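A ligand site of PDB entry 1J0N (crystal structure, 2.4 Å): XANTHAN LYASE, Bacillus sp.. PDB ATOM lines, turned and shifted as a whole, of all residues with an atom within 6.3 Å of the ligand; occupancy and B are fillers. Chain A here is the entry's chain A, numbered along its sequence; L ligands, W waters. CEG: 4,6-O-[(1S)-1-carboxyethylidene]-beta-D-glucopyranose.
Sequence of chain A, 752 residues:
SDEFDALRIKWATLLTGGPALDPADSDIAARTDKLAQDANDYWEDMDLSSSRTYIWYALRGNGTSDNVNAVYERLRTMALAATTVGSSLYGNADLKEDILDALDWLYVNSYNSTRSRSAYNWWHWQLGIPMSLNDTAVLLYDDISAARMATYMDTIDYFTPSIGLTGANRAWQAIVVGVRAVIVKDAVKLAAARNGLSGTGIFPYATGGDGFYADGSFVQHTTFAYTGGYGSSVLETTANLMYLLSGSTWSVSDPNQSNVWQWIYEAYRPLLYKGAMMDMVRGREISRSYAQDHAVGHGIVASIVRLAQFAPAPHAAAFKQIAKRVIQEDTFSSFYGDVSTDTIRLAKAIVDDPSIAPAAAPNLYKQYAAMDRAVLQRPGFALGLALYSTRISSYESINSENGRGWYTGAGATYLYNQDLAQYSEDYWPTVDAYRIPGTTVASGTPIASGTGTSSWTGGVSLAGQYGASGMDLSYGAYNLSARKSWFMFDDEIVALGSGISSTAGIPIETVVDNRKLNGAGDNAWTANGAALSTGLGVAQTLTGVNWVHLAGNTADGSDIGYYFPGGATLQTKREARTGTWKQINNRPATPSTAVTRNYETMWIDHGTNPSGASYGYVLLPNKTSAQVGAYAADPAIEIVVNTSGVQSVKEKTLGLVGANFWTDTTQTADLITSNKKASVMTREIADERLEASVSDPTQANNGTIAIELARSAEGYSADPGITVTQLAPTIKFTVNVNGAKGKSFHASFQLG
Merely in contact with the ligand: Trp 123 (3.4 Å) and Glu 285 (3.7 Å). Of the 20 residues printed, 8 come within 4 Å of the ligand.
NH1 of Arg 284 lies within hydrogen-bond range of OH of Tyr 230 (3.1 Å). NE2 of His 221 sits close to OH of Tyr 230 (3.3 Å). The side-chain hydroxyl (OH) of Tyr 290 sits at hydrogen-bond distance from the guanidinium group (NH1) of Arg 587 (3.3 Å). NH1 of Arg 587 is in salt-bridge range of OE2 of Glu 401 (2.8 Å). The side-chain carboxylate of Glu 285 is in salt-bridge range of the guanidinium group of Arg 288 (3.9 Å). The guanidinium group of Arg 288 lies within salt-bridge range of the side-chain carboxylate of Glu 401, at 2.9 Å. The guanidinium group of Arg 284 lies within salt-bridge range of the side-chain carboxylate of Glu 401, at 2.6 Å. The backbone carbonyl oxygen (O) of Trp 123 is in hydrogen-bond range of the backbone NH (N) of Gly 128.
Water W4 lies within hydrogen-bond range of O2 of the ligand (2.5 Å), OE2 of Glu 285 (2.8 Å) and NH1 of Arg 284 (3.5 Å). Water W5 bridges O8B of the ligand and OH of Tyr 290. Water W6 bridges OH of Tyr 230 (2.7 Å) and O1 of the ligand (2.7 Å). Water W1 lies within hydrogen-bond range of a ring nitrogen (NE2) of His 124 (2.8 Å), an oxygen (O6) of the ligand (2.9 Å) and the guanidinium group of Arg 587 (3.2 Å). Water W2 lies within hydrogen-bond range of the side-chain carboxylate of Glu 285 (2.8 Å), the side-chain hydroxyl of Ser 233 (2.9 Å) and an oxygen (O3) of the ligand (3.0 Å).
The side-chain hydroxyl (OH) of Tyr 230 is in hydrogen-bond range of an oxygen (O1) of the ligand (2.7 Å). An oxygen (O8B) of the ligand is in salt-bridge range of the guanidinium group of Arg 587 (2.7 Å). The side-chain hydroxyl (OH) of Tyr 290 is in hydrogen-bond range of an oxygen (O8A) of the ligand, 2.9 Å away. The guanidinium group of Arg 288 is in salt-bridge range of an oxygen (O8A) of the ligand (3.1 Å). The guanidinium group (NH2) of Arg 284 sits close to an oxygen (O1) of the ligand (3.2 Å). NE2 of His 124 sits at hydrogen-bond distance from O6 of the ligand (3.4 Å).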
ATOM      1  N   ASN A  69     -16.923 -19.815  -2.541  1.00  0.00           N
ATOM      2  CA  ASN A  69     -17.835 -18.688  -2.454  1.00  0.00           C
ATOM      3  C   ASN A  69     -17.268 -17.524  -3.244  1.00  0.00           C
ATOM      4  O   ASN A  69     -18.005 -16.812  -3.929  1.00  0.00           O
ATOM      5  CB  ASN A  69     -18.026 -18.290  -0.984  1.00  0.00           C
ATOM      6  CG  ASN A  69     -19.114 -17.243  -0.805  1.00  0.00           C
ATOM      7  OD1 ASN A  69     -18.825 -16.061  -0.615  1.00  0.00           O
ATOM      8  ND2 ASN A  69     -20.367 -17.669  -0.883  1.00  0.00           N
ATOM      9  N   GLU A  73     -18.626 -15.236  -6.641  1.00  0.00           N
ATOM     10  CA  GLU A  73     -18.749 -13.781  -6.628  1.00  0.00           C
ATOM     11  C   GLU A  73     -18.040 -13.207  -7.839  1.00  0.00           C
ATOM     12  O   GLU A  73     -18.568 -12.332  -8.526  1.00  0.00           O
ATOM     13  CB  GLU A  73     -18.163 -13.189  -5.341  1.00  0.00           C
ATOM     14  CG  GLU A  73     -19.024 -13.444  -4.107  1.00  0.00           C
ATOM     15  CD  GLU A  73     -18.453 -12.836  -2.824  1.00  0.00           C
ATOM     16  OE1 GLU A  73     -17.304 -13.177  -2.468  1.00  0.00           O
ATOM     17  OE2 GLU A  73     -19.155 -12.043  -2.164  1.00  0.00           O
ATOM     18  N   ASN A 121     -19.118 -24.324   7.218  1.00  0.00           N
ATOM     19  CA  ASN A 121     -19.645 -23.039   6.801  1.00  0.00           C
ATOM     20  C   ASN A 121     -20.766 -23.267   5.831  1.00  0.00           C
ATOM     21  O   ASN A 121     -20.620 -23.150   4.604  1.00  0.00           O
ATOM     22  CB  ASN A 121     -18.560 -22.150   6.195  1.00  0.00           C
ATOM     23  CG  ASN A 121     -18.472 -20.801   6.895  1.00  0.00           C
ATOM     24  OD1 ASN A 121     -19.497 -20.190   7.224  1.00  0.00           O
ATOM     25  ND2 ASN A 121     -17.265 -20.335   7.134  1.00  0.00           N
ATOM     26  N   TRP A 123     -23.256 -21.479   5.718  1.00  0.00           N
ATOM     27  CA  TRP A 123     -23.645 -20.190   5.192  1.00  0.00           C
ATOM     28  C   TRP A 123     -23.239 -20.095   3.725  1.00  0.00           C
ATOM     29  O   TRP A 123     -24.027 -19.641   2.895  1.00  0.00           O
ATOM     30  CB  TRP A 123     -23.006 -19.046   5.972  1.00  0.00           C
ATOM     31  CG  TRP A 123     -23.644 -17.750   5.600  1.00  0.00           C
ATOM     32  CD1 TRP A 123     -24.758 -17.187   6.167  1.00  0.00           C
ATOM     33  CD2 TRP A 123     -23.284 -16.908   4.502  1.00  0.00           C
ATOM     34  NE1 TRP A 123     -25.117 -16.058   5.474  1.00  0.00           N
ATOM     35  CE2 TRP A 123     -24.225 -15.854   4.454  1.00  0.00           C
ATOM     36  CE3 TRP A 123     -22.253 -16.929   3.550  1.00  0.00           C
ATOM     37  CZ2 TRP A 123     -24.171 -14.841   3.485  1.00  0.00           C
ATOM     38  CZ3 TRP A 123     -22.196 -15.924   2.592  1.00  0.00           C
ATOM     39  CH2 TRP A 123     -23.154 -14.887   2.564  1.00  0.00           C
ATOM     40  N   HIS A 124     -22.016 -20.510   3.424  1.00  0.00           N
ATOM     41  CA  HIS A 124     -21.536 -20.477   2.044  1.00  0.00           C
ATOM     42  C   HIS A 124     -22.285 -21.489   1.167  1.00  0.00           C
ATOM     43  O   HIS A 124     -22.782 -21.153   0.093  1.00  0.00           O
ATOM     44  CB  HIS A 124     -20.037 -20.803   2.008  1.00  0.00           C
ATOM     45  CG  HIS A 124     -19.164 -19.692   2.490  1.00  0.00           C
ATOM     46  ND1 HIS A 124     -17.975 -19.916   3.155  1.00  0.00           N
ATOM     47  CD2 HIS A 124     -19.284 -18.348   2.387  1.00  0.00           C
ATOM     48  CE1 HIS A 124     -17.403 -18.759   3.433  1.00  0.00           C
ATOM     49  NE2 HIS A 124     -18.181 -17.793   2.981  1.00  0.00           N
ATOM     50  N   GLY A 128     -24.609 -18.085   0.665  1.00  0.00           N
ATOM     51  CA  GLY A 128     -23.668 -17.332  -0.151  1.00  0.00           C
ATOM     52  C   GLY A 128     -23.524 -17.754  -1.598  1.00  0.00           C
ATOM     53  O   GLY A 128     -23.666 -16.934  -2.493  1.00  0.00           O
ATOM     54  N   ASN A 169     -30.658 -14.821   8.764  1.00  0.00           N
ATOM     55  CA  ASN A 169     -30.576 -16.099   8.077  1.00  0.00           C
ATOM     56  C   ASN A 169     -31.881 -16.442   7.357  1.00  0.00           C
ATOM     57  O   ASN A 169     -31.874 -16.829   6.184  1.00  0.00           O
ATOM     58  CB  ASN A 169     -30.171 -17.209   9.045  1.00  0.00           C
ATOM     59  CG  ASN A 169     -28.752 -17.037   9.561  1.00  0.00           C
ATOM     60  OD1 ASN A 169     -27.839 -16.739   8.792  1.00  0.00           O
ATOM     61  ND2 ASN A 169     -28.560 -17.223  10.870  1.00  0.00           N
ATOM     62  N   TRP A 172     -32.266 -14.401   4.274  1.00  0.00           N
ATOM     63  CA  TRP A 172     -31.375 -14.864   3.212  1.00  0.00           C
ATOM     64  C   TRP A 172     -31.936 -16.116   2.541  1.00  0.00           C
ATOM     65  O   TRP A 172     -31.801 -16.284   1.336  1.00  0.00           O
ATOM     66  CB  TRP A 172     -29.980 -15.190   3.747  1.00  0.00           C
ATOM     67  CG  TRP A 172     -29.054 -14.025   3.819  1.00  0.00           C
ATOM     68  CD1 TRP A 172     -28.841 -13.082   2.852  1.00  0.00           C
ATOM     69  CD2 TRP A 172     -28.148 -13.714   4.894  1.00  0.00           C
ATOM     70  NE1 TRP A 172     -27.849 -12.209   3.257  1.00  0.00           N
ATOM     71  CE2 TRP A 172     -27.407 -12.574   4.498  1.00  0.00           C
ATOM     72  CE3 TRP A 172     -27.881 -14.295   6.138  1.00  0.00           C
ATOM     73  CZ2 TRP A 172     -26.424 -12.003   5.308  1.00  0.00           C
ATOM     74  CZ3 TRP A 172     -26.898 -13.724   6.949  1.00  0.00           C
ATOM     75  CH2 TRP A 172     -26.186 -12.590   6.531  1.00  0.00           C
ATOM     76  N   HIS A 221     -27.910 -13.895  16.759  1.00  0.00           N
ATOM     77  CA  HIS A 221     -27.098 -14.858  17.497  1.00  0.00           C
ATOM     78  C   HIS A 221     -27.451 -14.791  18.985  1.00  0.00           C
ATOM     79  O   HIS A 221     -26.611 -15.020  19.848  1.00  0.00           O
ATOM     80  CB  HIS A 221     -25.602 -14.634  17.268  1.00  0.00           C
ATOM     81  CG  HIS A 221     -25.124 -15.170  15.945  1.00  0.00           C
ATOM     82  ND1 HIS A 221     -23.829 -15.008  15.499  1.00  0.00           N
ATOM     83  CD2 HIS A 221     -25.775 -15.873  14.987  1.00  0.00           C
ATOM     84  CE1 HIS A 221     -23.704 -15.588  14.317  1.00  0.00           C
ATOM     85  NE2 HIS A 221     -24.869 -16.116  13.981  1.00  0.00           N
ATOM     86  N   TYR A 226     -26.754  -6.297  16.912  1.00  0.00           N
ATOM     87  CA  TYR A 226     -26.246  -6.369  15.547  1.00  0.00           C
ATOM     88  C   TYR A 226     -26.891  -5.458  14.510  1.00  0.00           C
ATOM     89  O   TYR A 226     -26.665  -5.652  13.316  1.00  0.00           O
ATOM     90  CB  TYR A 226     -26.351  -7.817  15.063  1.00  0.00           C
ATOM     91  CG  TYR A 226     -25.028  -8.515  14.932  1.00  0.00           C
ATOM     92  CD1 TYR A 226     -24.104  -8.121  13.955  1.00  0.00           C
ATOM     93  CD2 TYR A 226     -24.670  -9.550  15.798  1.00  0.00           C
ATOM     94  CE1 TYR A 226     -22.868  -8.753  13.843  1.00  0.00           C
ATOM     95  CE2 TYR A 226     -23.437 -10.176  15.699  1.00  0.00           C
ATOM     96  CZ  TYR A 226     -22.536  -9.778  14.721  1.00  0.00           C
ATOM     97  OH  TYR A 226     -21.298 -10.387  14.631  1.00  0.00           O
ATOM     98  N   GLY A 229     -24.866  -4.917  11.612  1.00  0.00           N
ATOM     99  CA  GLY A 229     -24.217  -6.091  11.022  1.00  0.00           C
ATOM    100  C   GLY A 229     -25.236  -6.981  10.329  1.00  0.00           C
ATOM    101  O   GLY A 229     -25.580  -6.761   9.172  1.00  0.00           O
ATOM    102  N   TYR A 230     -25.709  -8.005  11.032  1.00  0.00           N
ATOM    103  CA  TYR A 230     -26.699  -8.909  10.466  1.00  0.00           C
ATOM    104  C   TYR A 230     -27.959  -8.080  10.187  1.00  0.00           C
ATOM    105  O   TYR A 230     -28.697  -8.359   9.246  1.00  0.00           O
ATOM    106  CB  TYR A 230     -27.036 -10.029  11.447  1.00  0.00           C
ATOM    107  CG  TYR A 230     -26.055 -11.172  11.474  1.00  0.00           C
ATOM    108  CD1 TYR A 230     -25.995 -12.078  10.414  1.00  0.00           C
ATOM    109  CD2 TYR A 230     -25.202 -11.365  12.547  1.00  0.00           C
ATOM    110  CE1 TYR A 230     -25.115 -13.163  10.436  1.00  0.00           C
ATOM    111  CE2 TYR A 230     -24.307 -12.443  12.593  1.00  0.00           C
ATOM    112  CZ  TYR A 230     -24.272 -13.337  11.521  1.00  0.00           C
ATOM    113  OH  TYR A 230     -23.395 -14.392  11.552  1.00  0.00           O
ATOM    114  N   SER A 233     -27.828  -6.620   6.817  1.00  0.00           N
ATOM    115  CA  SER A 233     -28.201  -7.608   5.806  1.00  0.00           C
ATOM    116  C   SER A 233     -29.705  -7.797   5.730  1.00  0.00           C
ATOM    117  O   SER A 233     -30.282  -7.788   4.654  1.00  0.00           O
ATOM    118  CB  SER A 233     -27.555  -8.954   6.114  1.00  0.00           C
ATOM    119  OG  SER A 233     -26.147  -8.871   6.037  1.00  0.00           O
ATOM    120  N   ARG A 284     -18.974  -8.454  15.034  1.00  0.00           N
ATOM    121  CA  ARG A 284     -17.656  -8.919  14.613  1.00  0.00           C
ATOM    122  C   ARG A 284     -17.255  -8.354  13.260  1.00  0.00           C
ATOM    123  O   ARG A 284     -16.114  -8.511  12.828  1.00  0.00           O
ATOM    124  CB  ARG A 284     -17.587 -10.457  14.583  1.00  0.00           C
ATOM    125  CG  ARG A 284     -18.242 -11.136  13.381  1.00  0.00           C
ATOM    126  CD  ARG A 284     -18.017 -12.655  13.448  1.00  0.00           C
ATOM    127  NE  ARG A 284     -18.404 -13.386  12.237  1.00  0.00           N
ATOM    128  CZ  ARG A 284     -19.646 -13.738  11.906  1.00  0.00           C
ATOM    129  NH1 ARG A 284     -20.666 -13.424  12.689  1.00  0.00           N
ATOM    130  NH2 ARG A 284     -19.870 -14.429  10.793  1.00  0.00           N
ATOM    131  N   GLU A 285     -18.191  -7.675  12.608  1.00  0.00           N
ATOM    132  CA  GLU A 285     -17.938  -7.101  11.299  1.00  0.00           C
ATOM    133  C   GLU A 285     -16.990  -5.914  11.319  1.00  0.00           C
ATOM    134  O   GLU A 285     -16.473  -5.519  10.265  1.00  0.00           O
ATOM    135  CB  GLU A 285     -19.265  -6.734  10.636  1.00  0.00           C
ATOM    136  CG  GLU A 285     -20.056  -7.971  10.184  1.00  0.00           C
ATOM    137  CD  GLU A 285     -21.305  -7.645   9.393  1.00  0.00           C
ATOM    138  OE1 GLU A 285     -21.271  -6.705   8.571  1.00  0.00           O
ATOM    139  OE2 GLU A 285     -22.325  -8.353   9.585  1.00  0.00           O
ATOM    140  N   ARG A 288     -13.759  -6.444   9.514  1.00  0.00           N
ATOM    141  CA  ARG A 288     -13.714  -6.622   8.058  1.00  0.00           C
ATOM    142  C   ARG A 288     -13.303  -5.335   7.339  1.00  0.00           C
ATOM    143  O   ARG A 288     -14.023  -4.338   7.376  1.00  0.00           O
ATOM    144  CB  ARG A 288     -15.078  -7.093   7.563  1.00  0.00           C
ATOM    145  CG  ARG A 288     -15.515  -8.399   8.195  1.00  0.00           C
ATOM    146  CD  ARG A 288     -16.943  -8.743   7.858  1.00  0.00           C
ATOM    147  NE  ARG A 288     -17.243 -10.110   8.267  1.00  0.00           N
ATOM    148  CZ  ARG A 288     -18.418 -10.707   8.112  1.00  0.00           C
ATOM    149  NH1 ARG A 288     -19.433 -10.057   7.548  1.00  0.00           N
ATOM    150  NH2 ARG A 288     -18.578 -11.955   8.520  1.00  0.00           N
ATOM    151  N   TYR A 290     -13.244  -4.573   4.145  1.00  0.00           N
ATOM    152  CA  TYR A 290     -14.137  -4.161   3.067  1.00  0.00           C
ATOM    153  C   TYR A 290     -15.464  -3.635   3.593  1.00  0.00           C
ATOM    154  O   TYR A 290     -16.325  -3.206   2.819  1.00  0.00           O
ATOM    155  CB  TYR A 290     -14.431  -5.335   2.137  1.00  0.00           C
ATOM    156  CG  TYR A 290     -14.815  -6.610   2.865  1.00  0.00           C
ATOM    157  CD1 TYR A 290     -13.839  -7.439   3.411  1.00  0.00           C
ATOM    158  CD2 TYR A 290     -16.146  -6.975   3.010  1.00  0.00           C
ATOM    159  CE1 TYR A 290     -14.183  -8.610   4.079  1.00  0.00           C
ATOM    160  CE2 TYR A 290     -16.504  -8.146   3.682  1.00  0.00           C
ATOM    161  CZ  TYR A 290     -15.524  -8.956   4.213  1.00  0.00           C
ATOM    162  OH  TYR A 290     -15.857 -10.098   4.887  1.00  0.00           O
ATOM    163  N   ASN A 399     -15.178 -17.886  13.763  1.00  0.00           N
ATOM    164  CA  ASN A 399     -14.536 -17.972  12.456  1.00  0.00           C
ATOM    165  C   ASN A 399     -13.275 -17.121  12.376  1.00  0.00           C
ATOM    166  O   ASN A 399     -12.972 -16.526  11.334  1.00  0.00           O
ATOM    167  CB  ASN A 399     -15.518 -17.527  11.370  1.00  0.00           C
ATOM    168  CG  ASN A 399     -16.698 -18.470  11.242  1.00  0.00           C
ATOM    169  OD1 ASN A 399     -17.799 -18.058  10.906  1.00  0.00           O
ATOM    170  ND2 ASN A 399     -16.455 -19.758  11.496  1.00  0.00           N
ATOM    171  N   GLU A 401     -12.531 -14.205  13.502  1.00  0.00           N
ATOM    172  CA  GLU A 401     -12.784 -12.815  13.167  1.00  0.00           C
ATOM    173  C   GLU A 401     -12.941 -12.042  14.477  1.00  0.00           C
ATOM    174  O   GLU A 401     -13.493 -12.563  15.434  1.00  0.00           O
ATOM    175  CB  GLU A 401     -14.080 -12.664  12.378  1.00  0.00           C
ATOM    176  CG  GLU A 401     -14.023 -13.093  10.934  1.00  0.00           C
ATOM    177  CD  GLU A 401     -15.314 -12.791  10.206  1.00  0.00           C
ATOM    178  OE1 GLU A 401     -16.359 -13.362  10.585  1.00  0.00           O
ATOM    179  OE2 GLU A 401     -15.287 -11.968   9.260  1.00  0.00           O
ATOM    180  N   ARG A 587      -8.471 -14.861   8.063  1.00  0.00           N
ATOM    181  CA  ARG A 587      -9.139 -15.642   7.039  1.00  0.00           C
ATOM    182  C   ARG A 587      -8.296 -15.539   5.773  1.00  0.00           C
ATOM    183  O   ARG A 587      -7.529 -14.579   5.600  1.00  0.00           O
ATOM    184  CB  ARG A 587     -10.547 -15.104   6.765  1.00  0.00           C
ATOM    185  CG  ARG A 587     -11.531 -15.313   7.898  1.00  0.00           C
ATOM    186  CD  ARG A 587     -12.510 -14.157   7.978  1.00  0.00           C
ATOM    187  NE  ARG A 587     -13.663 -14.279   7.103  1.00  0.00           N
ATOM    188  CZ  ARG A 587     -14.317 -13.246   6.582  1.00  0.00           C
ATOM    189  NH1 ARG A 587     -13.932 -12.001   6.834  1.00  0.00           N
ATOM    190  NH2 ARG A 587     -15.383 -13.455   5.818  1.00  0.00           N
HETATM  191  C1  CEG L   1     -21.720 -14.222   8.146  1.00  0.00           C
HETATM  192  C2  CEG L   1     -22.312 -12.860   7.741  1.00  0.00           C
HETATM  193  C3  CEG L   1     -22.052 -12.481   6.250  1.00  0.00           C
HETATM  194  C4  CEG L   1     -20.776 -13.161   5.732  1.00  0.00           C
HETATM  195  C5  CEG L   1     -20.902 -14.717   5.794  1.00  0.00           C
HETATM  196  C6  CEG L   1     -19.756 -15.085   5.347  1.00  0.00           C
HETATM  197  C7  CEG L   1     -19.303 -13.225   3.910  1.00  0.00           C
HETATM  198  C8  CEG L   1     -18.251 -12.308   4.208  1.00  0.00           C
HETATM  199  C9  CEG L   1     -19.672 -13.438   2.383  1.00  0.00           C
HETATM  200  O1  CEG L   1     -22.572 -14.837   9.035  1.00  0.00           O
HETATM  201  O2  CEG L   1     -21.752 -11.871   8.586  1.00  0.00           O
HETATM  202  O3  CEG L   1     -21.896 -11.066   6.141  1.00  0.00           O
HETATM  203  O4  CEG L   1     -20.577 -12.731   4.346  1.00  0.00           O
HETATM  204  O5  CEG L   1     -21.566 -15.142   7.053  1.00  0.00           O
HETATM  205  O6  CEG L   1     -19.094 -14.712   4.142  1.00  0.00           O
HETATM  206  O8A CEG L   1     -18.490 -11.224   4.781  1.00  0.00           O
HETATM  207  O8B CEG L   1     -17.110 -12.699   3.850  1.00  0.00           O
HETATM  208  O   HOH W   1     -16.429 -15.766   3.923  1.00  0.00           O
HETATM  209  O   HOH W   2     -23.929  -9.657   7.749  1.00  0.00           O
HETATM  210  O   HOH W   3     -20.248  -9.636   3.564  1.00  0.00           O
HETATM  211  O   HOH W   4     -22.124 -10.872  10.846  1.00  0.00           O
HETATM  212  O   HOH W   5     -15.056 -12.060   2.226  1.00  0.00           O
HETATM  213  O   HOH W   6     -24.183 -16.679  10.274  1.00  0.00           O
